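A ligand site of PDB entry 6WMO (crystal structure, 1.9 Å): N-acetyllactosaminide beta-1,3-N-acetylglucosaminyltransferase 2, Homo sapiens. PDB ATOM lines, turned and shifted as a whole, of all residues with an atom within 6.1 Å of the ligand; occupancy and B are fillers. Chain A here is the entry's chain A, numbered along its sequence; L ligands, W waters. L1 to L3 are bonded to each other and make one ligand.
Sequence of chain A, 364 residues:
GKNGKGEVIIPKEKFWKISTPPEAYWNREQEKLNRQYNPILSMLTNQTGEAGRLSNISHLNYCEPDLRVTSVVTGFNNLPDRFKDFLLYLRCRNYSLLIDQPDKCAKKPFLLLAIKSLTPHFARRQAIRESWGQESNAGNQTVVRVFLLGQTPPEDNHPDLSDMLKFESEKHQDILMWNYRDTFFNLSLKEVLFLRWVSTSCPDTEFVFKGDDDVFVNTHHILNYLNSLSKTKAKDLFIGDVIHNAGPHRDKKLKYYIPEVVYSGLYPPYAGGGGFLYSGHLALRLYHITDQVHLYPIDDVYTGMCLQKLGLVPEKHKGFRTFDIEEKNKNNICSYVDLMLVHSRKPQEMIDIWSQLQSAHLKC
An oxygen (O2) of LG3 L3 is in hydrogen-bond range of the side-chain carboxylate (OD2) of Asp 300, 2.7 Å away.
OH of Tyr 270 is in hydrogen-bond range of O1 of LG2 L2.
O4 of LG2 L2 is in hydrogen-bond range of NE2 of His 249, at 3.1 Å.
O of Tyr 270 lies within hydrogen-bond range of N of Ile 243, 2.9 Å away.
The side-chain carboxylate (OD2) of Asp 300 is in hydrogen-bond range of the backbone NH (N) of Gly 273 (2.9 Å).
N of Tyr 267 lies within hydrogen-bond range of O of Ala 246, 2.9 Å away.
Residues that only touch the ligand: Ile 243 (3.7 Å), His 244 (3.9 Å), Ala 246 (3.7 Å), Tyr 256 (3.5 Å), Ile 298 (3.6 Å) and Phe 323 (3.4 Å).
Hydrophobic or aromatic side chains that line the ligand: Ile 243, Ala 246, His 249, Tyr 256, Tyr 270, Ile 298 and Phe 323.
Nine residues have an atom within 4 Å of the ligand: Ile 243, His 244, Ala 246, His 249, Tyr 256, Tyr 270, Ile 298, Asp 300 and Phe 323.
Water W2 lies within hydrogen-bond range of O of Tyr 256 (2.7 Å), O5 of LG3 L3 (2.7 Å), OH of Tyr 267 (2.8 Å) and N of His 249 (3.2 Å).
Water W3 lies within hydrogen-bond range of the backbone carbonyl oxygen of Gly 247 and an oxygen (O5) of LG3 L3.
Water W1 lies within hydrogen-bond range of a nitrogen (N1) of LG2 L2 (2.9 Å) and the backbone NH (N) of Gly 247 (3.2 Å).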
ATOM      1  N   ILE A 243      23.227  11.410  19.918  1.00  0.00           N
ATOM      2  CA  ILE A 243      22.160  12.170  20.538  1.00  0.00           C
ATOM      3  C   ILE A 243      21.333  11.207  21.383  1.00  0.00           C
ATOM      4  O   ILE A 243      20.843  10.196  20.863  1.00  0.00           O
ATOM      5  CB  ILE A 243      21.289  12.871  19.476  1.00  0.00           C
ATOM      6  CG1 ILE A 243      22.156  13.807  18.616  1.00  0.00           C
ATOM      7  CG2 ILE A 243      20.140  13.618  20.139  1.00  0.00           C
ATOM      8  CD1 ILE A 243      21.616  14.122  17.190  1.00  0.00           C
ATOM      9  N   HIS A 244      21.227  11.492  22.669  1.00  0.00           N
ATOM     10  CA  HIS A 244      20.421  10.703  23.585  1.00  0.00           C
ATOM     11  C   HIS A 244      19.120  11.434  23.921  1.00  0.00           C
ATOM     12  O   HIS A 244      19.063  12.658  23.931  1.00  0.00           O
ATOM     13  CB  HIS A 244      21.180  10.390  24.880  1.00  0.00           C
ATOM     14  CG  HIS A 244      22.189   9.304  24.743  1.00  0.00           C
ATOM     15  ND1 HIS A 244      23.490   9.527  24.357  1.00  0.00           N
ATOM     16  CD2 HIS A 244      22.088   7.967  24.971  1.00  0.00           C
ATOM     17  CE1 HIS A 244      24.151   8.387  24.333  1.00  0.00           C
ATOM     18  NE2 HIS A 244      23.321   7.427  24.704  1.00  0.00           N
ATOM     19  N   ASN A 245      18.079  10.641  24.212  1.00  0.00           N
ATOM     20  CA  ASN A 245      16.794  11.151  24.672  1.00  0.00           C
ATOM     21  C   ASN A 245      16.157  12.111  23.665  1.00  0.00           C
ATOM     22  O   ASN A 245      15.481  13.066  24.046  1.00  0.00           O
ATOM     23  CB  ASN A 245      16.915  11.833  26.049  1.00  0.00           C
ATOM     24  CG  ASN A 245      17.572  10.949  27.076  1.00  0.00           C
ATOM     25  OD1 ASN A 245      17.283   9.753  27.157  1.00  0.00           O
ATOM     26  ND2 ASN A 245      18.464  11.514  27.873  1.00  0.00           N
ATOM     27  N   ALA A 246      16.375  11.867  22.378  1.00  0.00           N
ATOM     28  CA  ALA A 246      15.735  12.673  21.346  1.00  0.00           C
ATOM     29  C   ALA A 246      14.387  12.077  20.975  1.00  0.00           C
ATOM     30  O   ALA A 246      14.109  10.898  21.217  1.00  0.00           O
ATOM     31  CB  ALA A 246      16.621  12.774  20.105  1.00  0.00           C
ATOM     32  N   GLY A 247      13.531  12.928  20.411  1.00  0.00           N
ATOM     33  CA  GLY A 247      12.247  12.533  19.897  1.00  0.00           C
ATOM     34  C   GLY A 247      11.992  13.187  18.557  1.00  0.00           C
ATOM     35  O   GLY A 247      12.763  14.045  18.108  1.00  0.00           O
ATOM     36  N   PRO A 248      10.917  12.798  17.884  1.00  0.00           N
ATOM     37  CA  PRO A 248      10.638  13.371  16.566  1.00  0.00           C
ATOM     38  C   PRO A 248      10.252  14.836  16.672  1.00  0.00           C
ATOM     39  O   PRO A 248       9.618  15.269  17.633  1.00  0.00           O
ATOM     40  CB  PRO A 248       9.471  12.522  16.052  1.00  0.00           C
ATOM     41  CG  PRO A 248       8.844  11.946  17.277  1.00  0.00           C
ATOM     42  CD  PRO A 248       9.944  11.754  18.262  1.00  0.00           C
ATOM     43  N   HIS A 249      10.692  15.622  15.683  1.00  0.00           N
ATOM     44  CA  HIS A 249      10.266  17.014  15.581  1.00  0.00           C
ATOM     45  C   HIS A 249       8.809  17.066  15.155  1.00  0.00           C
ATOM     46  O   HIS A 249       8.427  16.450  14.167  1.00  0.00           O
ATOM     47  CB  HIS A 249      11.146  17.772  14.579  1.00  0.00           C
ATOM     48  CG  HIS A 249      12.470  18.198  15.122  1.00  0.00           C
ATOM     49  ND1 HIS A 249      12.603  19.176  16.073  1.00  0.00           N
ATOM     50  CD2 HIS A 249      13.725  17.749  14.864  1.00  0.00           C
ATOM     51  CE1 HIS A 249      13.883  19.326  16.370  1.00  0.00           C
ATOM     52  NE2 HIS A 249      14.582  18.474  15.655  1.00  0.00           N
ATOM     53  N   LEU A 254       9.973  22.387  10.048  1.00  0.00           N
ATOM     54  CA  LEU A 254      11.302  21.809  10.011  1.00  0.00           C
ATOM     55  C   LEU A 254      11.376  20.646   9.029  1.00  0.00           C
ATOM     56  O   LEU A 254      10.412  19.896   8.858  1.00  0.00           O
ATOM     57  CB  LEU A 254      11.730  21.329  11.403  1.00  0.00           C
ATOM     58  CG  LEU A 254      11.936  22.369  12.497  1.00  0.00           C
ATOM     59  CD1 LEU A 254      12.192  21.681  13.825  1.00  0.00           C
ATOM     60  CD2 LEU A 254      13.096  23.286  12.132  1.00  0.00           C
ATOM     61  N   TYR A 256      12.896  17.942   9.321  1.00  0.00           N
ATOM     62  CA  TYR A 256      12.829  16.682  10.051  1.00  0.00           C
ATOM     63  C   TYR A 256      11.453  16.438  10.673  1.00  0.00           C
ATOM     64  O   TYR A 256      11.329  15.559  11.531  1.00  0.00           O
ATOM     65  CB  TYR A 256      13.897  16.640  11.136  1.00  0.00           C
ATOM     66  CG  TYR A 256      15.269  17.108  10.685  1.00  0.00           C
ATOM     67  CD1 TYR A 256      15.950  16.447   9.669  1.00  0.00           C
ATOM     68  CD2 TYR A 256      15.867  18.211  11.290  1.00  0.00           C
ATOM     69  CE1 TYR A 256      17.219  16.897   9.252  1.00  0.00           C
ATOM     70  CE2 TYR A 256      17.124  18.651  10.892  1.00  0.00           C
ATOM     71  CZ  TYR A 256      17.795  17.990   9.875  1.00  0.00           C
ATOM     72  OH  TYR A 256      19.043  18.442   9.493  1.00  0.00           O
ATOM     73  N   TYR A 267      13.057   8.484  20.041  1.00  0.00           N
ATOM     74  CA  TYR A 267      14.110   7.914  19.220  1.00  0.00           C
ATOM     75  C   TYR A 267      15.142   7.212  20.091  1.00  0.00           C
ATOM     76  O   TYR A 267      15.422   7.667  21.206  1.00  0.00           O
ATOM     77  CB  TYR A 267      14.809   9.004  18.402  1.00  0.00           C
ATOM     78  CG  TYR A 267      14.019   9.580  17.261  1.00  0.00           C
ATOM     79  CD1 TYR A 267      12.981   8.885  16.664  1.00  0.00           C
ATOM     80  CD2 TYR A 267      14.313  10.842  16.761  1.00  0.00           C
ATOM     81  CE1 TYR A 267      12.265   9.431  15.609  1.00  0.00           C
ATOM     82  CE2 TYR A 267      13.608  11.402  15.708  1.00  0.00           C
ATOM     83  CZ  TYR A 267      12.588  10.688  15.138  1.00  0.00           C
ATOM     84  OH  TYR A 267      11.893  11.248  14.086  1.00  0.00           O
ATOM     85  N   TYR A 270      21.318   7.741  18.721  1.00  0.00           N
ATOM     86  CA  TYR A 270      21.783   7.598  17.357  1.00  0.00           C
ATOM     87  C   TYR A 270      22.842   8.662  17.066  1.00  0.00           C
ATOM     88  O   TYR A 270      22.784   9.784  17.584  1.00  0.00           O
ATOM     89  CB  TYR A 270      20.633   7.697  16.326  1.00  0.00           C
ATOM     90  CG  TYR A 270      20.049   9.106  16.182  1.00  0.00           C
ATOM     91  CD1 TYR A 270      19.070   9.551  17.059  1.00  0.00           C
ATOM     92  CD2 TYR A 270      20.472   9.967  15.175  1.00  0.00           C
ATOM     93  CE1 TYR A 270      18.529  10.802  16.957  1.00  0.00           C
ATOM     94  CE2 TYR A 270      19.934  11.262  15.066  1.00  0.00           C
ATOM     95  CZ  TYR A 270      18.961  11.660  15.965  1.00  0.00           C
ATOM     96  OH  TYR A 270      18.399  12.905  15.903  1.00  0.00           O
ATOM     97  N   GLY A 272      24.421  11.340  14.617  1.00  0.00           N
ATOM     98  CA  GLY A 272      24.007  12.183  13.505  1.00  0.00           C
ATOM     99  C   GLY A 272      24.701  11.786  12.223  1.00  0.00           C
ATOM    100  O   GLY A 272      25.895  11.458  12.209  1.00  0.00           O
ATOM    101  N   GLY A 273      23.943  11.824  11.128  1.00  0.00           N
ATOM    102  CA  GLY A 273      24.360  11.250   9.865  1.00  0.00           C
ATOM    103  C   GLY A 273      25.464  11.993   9.154  1.00  0.00           C
ATOM    104  O   GLY A 273      26.014  11.433   8.196  1.00  0.00           O
ATOM    105  N   GLY A 274      25.775  13.225   9.568  1.00  0.00           N
ATOM    106  CA  GLY A 274      26.855  13.958   8.926  1.00  0.00           C
ATOM    107  C   GLY A 274      28.110  13.107   8.812  1.00  0.00           C
ATOM    108  O   GLY A 274      28.880  13.237   7.854  1.00  0.00           O
ATOM    109  N   ILE A 298      13.935   9.303   8.449  1.00  0.00           N
ATOM    110  CA  ILE A 298      15.191   9.921   8.874  1.00  0.00           C
ATOM    111  C   ILE A 298      16.260   8.826   8.919  1.00  0.00           C
ATOM    112  O   ILE A 298      16.167   7.898   9.728  1.00  0.00           O
ATOM    113  CB  ILE A 298      15.062  10.609  10.237  1.00  0.00           C
ATOM    114  CG1 ILE A 298      13.811  11.511  10.302  1.00  0.00           C
ATOM    115  CG2 ILE A 298      16.311  11.421  10.521  1.00  0.00           C
ATOM    116  CD1 ILE A 298      13.905  12.720   9.436  1.00  0.00           C
ATOM    117  N   ASP A 299      17.303   8.953   8.085  1.00  0.00           N
ATOM    118  CA  ASP A 299      18.174   7.794   7.885  1.00  0.00           C
ATOM    119  C   ASP A 299      19.048   7.541   9.104  1.00  0.00           C
ATOM    120  O   ASP A 299      19.297   6.372   9.444  1.00  0.00           O
ATOM    121  CB  ASP A 299      19.023   7.984   6.626  1.00  0.00           C
ATOM    122  CG  ASP A 299      20.060   9.127   6.748  1.00  0.00           C
ATOM    123  OD1 ASP A 299      19.761  10.153   7.401  1.00  0.00           O
ATOM    124  OD2 ASP A 299      21.163   9.014   6.153  1.00  0.00           O
ATOM    125  N   ASP A 300      19.539   8.575   9.792  1.00  0.00           N
ATOM    126  CA  ASP A 300      20.418   8.294  10.921  1.00  0.00           C
ATOM    127  C   ASP A 300      19.633   7.760  12.122  1.00  0.00           C
ATOM    128  O   ASP A 300      20.208   7.008  12.914  1.00  0.00           O
ATOM    129  CB  ASP A 300      21.284   9.517  11.274  1.00  0.00           C
ATOM    130  CG  ASP A 300      20.482  10.777  11.552  1.00  0.00           C
ATOM    131  OD1 ASP A 300      19.246  10.775  11.447  1.00  0.00           O
ATOM    132  OD2 ASP A 300      21.134  11.803  11.869  1.00  0.00           O
ATOM    133  N   VAL A 301      18.343   8.096  12.239  1.00  0.00           N
ATOM    134  CA  VAL A 301      17.506   7.430  13.237  1.00  0.00           C
ATOM    135  C   VAL A 301      17.353   5.955  12.895  1.00  0.00           C
ATOM    136  O   VAL A 301      17.368   5.082  13.791  1.00  0.00           O
ATOM    137  CB  VAL A 301      16.126   8.121  13.339  1.00  0.00           C
ATOM    138  CG1 VAL A 301      15.119   7.288  14.243  1.00  0.00           C
ATOM    139  CG2 VAL A 301      16.279   9.566  13.827  1.00  0.00           C
ATOM    140  N   THR A 322      28.971  17.731  14.412  1.00  0.00           N
ATOM    141  CA  THR A 322      27.929  17.757  13.377  1.00  0.00           C
ATOM    142  C   THR A 322      27.068  19.006  13.462  1.00  0.00           C
ATOM    143  O   THR A 322      26.243  19.235  12.573  1.00  0.00           O
ATOM    144  CB  THR A 322      27.066  16.505  13.477  1.00  0.00           C
ATOM    145  OG1 THR A 322      26.334  16.481  14.705  1.00  0.00           O
ATOM    146  CG2 THR A 322      27.948  15.261  13.401  1.00  0.00           C
ATOM    147  N   PHE A 323      27.261  19.811  14.505  1.00  0.00           N
ATOM    148  CA  PHE A 323      26.618  21.111  14.648  1.00  0.00           C
ATOM    149  C   PHE A 323      27.642  22.232  14.637  1.00  0.00           C
ATOM    150  O   PHE A 323      27.391  23.316  15.186  1.00  0.00           O
ATOM    151  CB  PHE A 323      25.754  21.127  15.917  1.00  0.00           C
ATOM    152  CG  PHE A 323      24.624  20.113  15.895  1.00  0.00           C
ATOM    153  CD1 PHE A 323      23.405  20.424  15.302  1.00  0.00           C
ATOM    154  CD2 PHE A 323      24.798  18.844  16.431  1.00  0.00           C
ATOM    155  CE1 PHE A 323      22.368  19.496  15.272  1.00  0.00           C
ATOM    156  CE2 PHE A 323      23.761  17.908  16.406  1.00  0.00           C
ATOM    157  CZ  PHE A 323      22.542  18.232  15.815  1.00  0.00           C
HETATM  158  C1  LIG L   1      16.129  22.333  21.837  1.00  0.00           C
HETATM  159  C2  LIG L   1      15.968  20.887  21.313  1.00  0.00           C
HETATM  160  C3  LIG L   1      16.738  20.650  20.003  1.00  0.00           C
HETATM  161  C4  LIG L   1      16.487  21.795  18.999  1.00  0.00           C
HETATM  162  C5  LIG L   1      16.717  23.157  19.687  1.00  0.00           C
HETATM  163  C6  LIG L   1      16.415  24.276  18.675  1.00  0.00           C
HETATM  164  O1  LIG L   1      15.191  22.518  22.905  1.00  0.00           O
HETATM  165  O2  LIG L   1      16.456  19.988  22.320  1.00  0.00           O
HETATM  166  O3  LIG L   1      16.256  19.434  19.424  1.00  0.00           O
HETATM  167  O4  LIG L   1      15.152  21.716  18.488  1.00  0.00           O
HETATM  168  O5  LIG L   1      15.843  23.254  20.810  1.00  0.00           O
HETATM  169  O6  LIG L   1      17.128  25.455  19.055  1.00  0.00           O
HETATM  170  C1  LG2 L   2      17.312  18.792  18.692  1.00  0.00           C
HETATM  171  C2  LG2 L   2      17.014  17.293  18.610  1.00  0.00           C
HETATM  172  C3  LG2 L   2      18.009  16.582  17.692  1.00  0.00           C
HETATM  173  C4  LG2 L   2      18.106  17.269  16.328  1.00  0.00           C
HETATM  174  C5  LG2 L   2      18.454  18.734  16.573  1.00  0.00           C
HETATM  175  C6  LG2 L   2      18.521  19.487  15.248  1.00  0.00           C
HETATM  176  C7  LG2 L   2      18.033  16.575  20.754  1.00  0.00           C
HETATM  177  C8  LG2 L   2      17.799  15.746  21.993  1.00  0.00           C
HETATM  178  N1  LG2 L   2      16.991  16.683  19.932  1.00  0.00           N
HETATM  179  O1  LG2 L   2      17.601  15.231  17.497  1.00  0.00           O
HETATM  180  O2  LG2 L   2      19.134  16.624  15.573  1.00  0.00           O
HETATM  181  O3  LG2 L   2      17.444  19.350  17.375  1.00  0.00           O
HETATM  182  O4  LG2 L   2      17.353  19.157  14.492  1.00  0.00           O
HETATM  183  O5  LG2 L   2      19.122  17.103  20.546  1.00  0.00           O
HETATM  184  C1  LG3 L   3      18.665  16.209  14.274  1.00  0.00           C
HETATM  185  C2  LG3 L   3      19.843  15.557  13.506  1.00  0.00           C
HETATM  186  C3  LG3 L   3      19.403  15.166  12.090  1.00  0.00           C
HETATM  187  C4  LG3 L   3      18.130  14.295  12.183  1.00  0.00           C
HETATM  188  C5  LG3 L   3      17.041  15.017  13.004  1.00  0.00           C
HETATM  189  C6  LG3 L   3      15.795  14.128  13.160  1.00  0.00           C
HETATM  190  O1  LG3 L   3      20.946  16.472  13.424  1.00  0.00           O
HETATM  191  O2  LG3 L   3      20.469  14.427  11.480  1.00  0.00           O
HETATM  192  O3  LG3 L   3      18.470  13.063  12.820  1.00  0.00           O
HETATM  193  O4  LG3 L   3      17.557  15.330  14.304  1.00  0.00           O
HETATM  194  O5  LG3 L   3      14.846  14.819  13.970  1.00  0.00           O
HETATM  195  O   HOH W   1      14.207  16.096  20.493  1.00  0.00           O
HETATM  196  O   HOH W   2      12.315  13.997  13.498  1.00  0.00           O
HETATM  197  O   HOH W   3      14.918  14.731  16.686  1.00  0.00           O
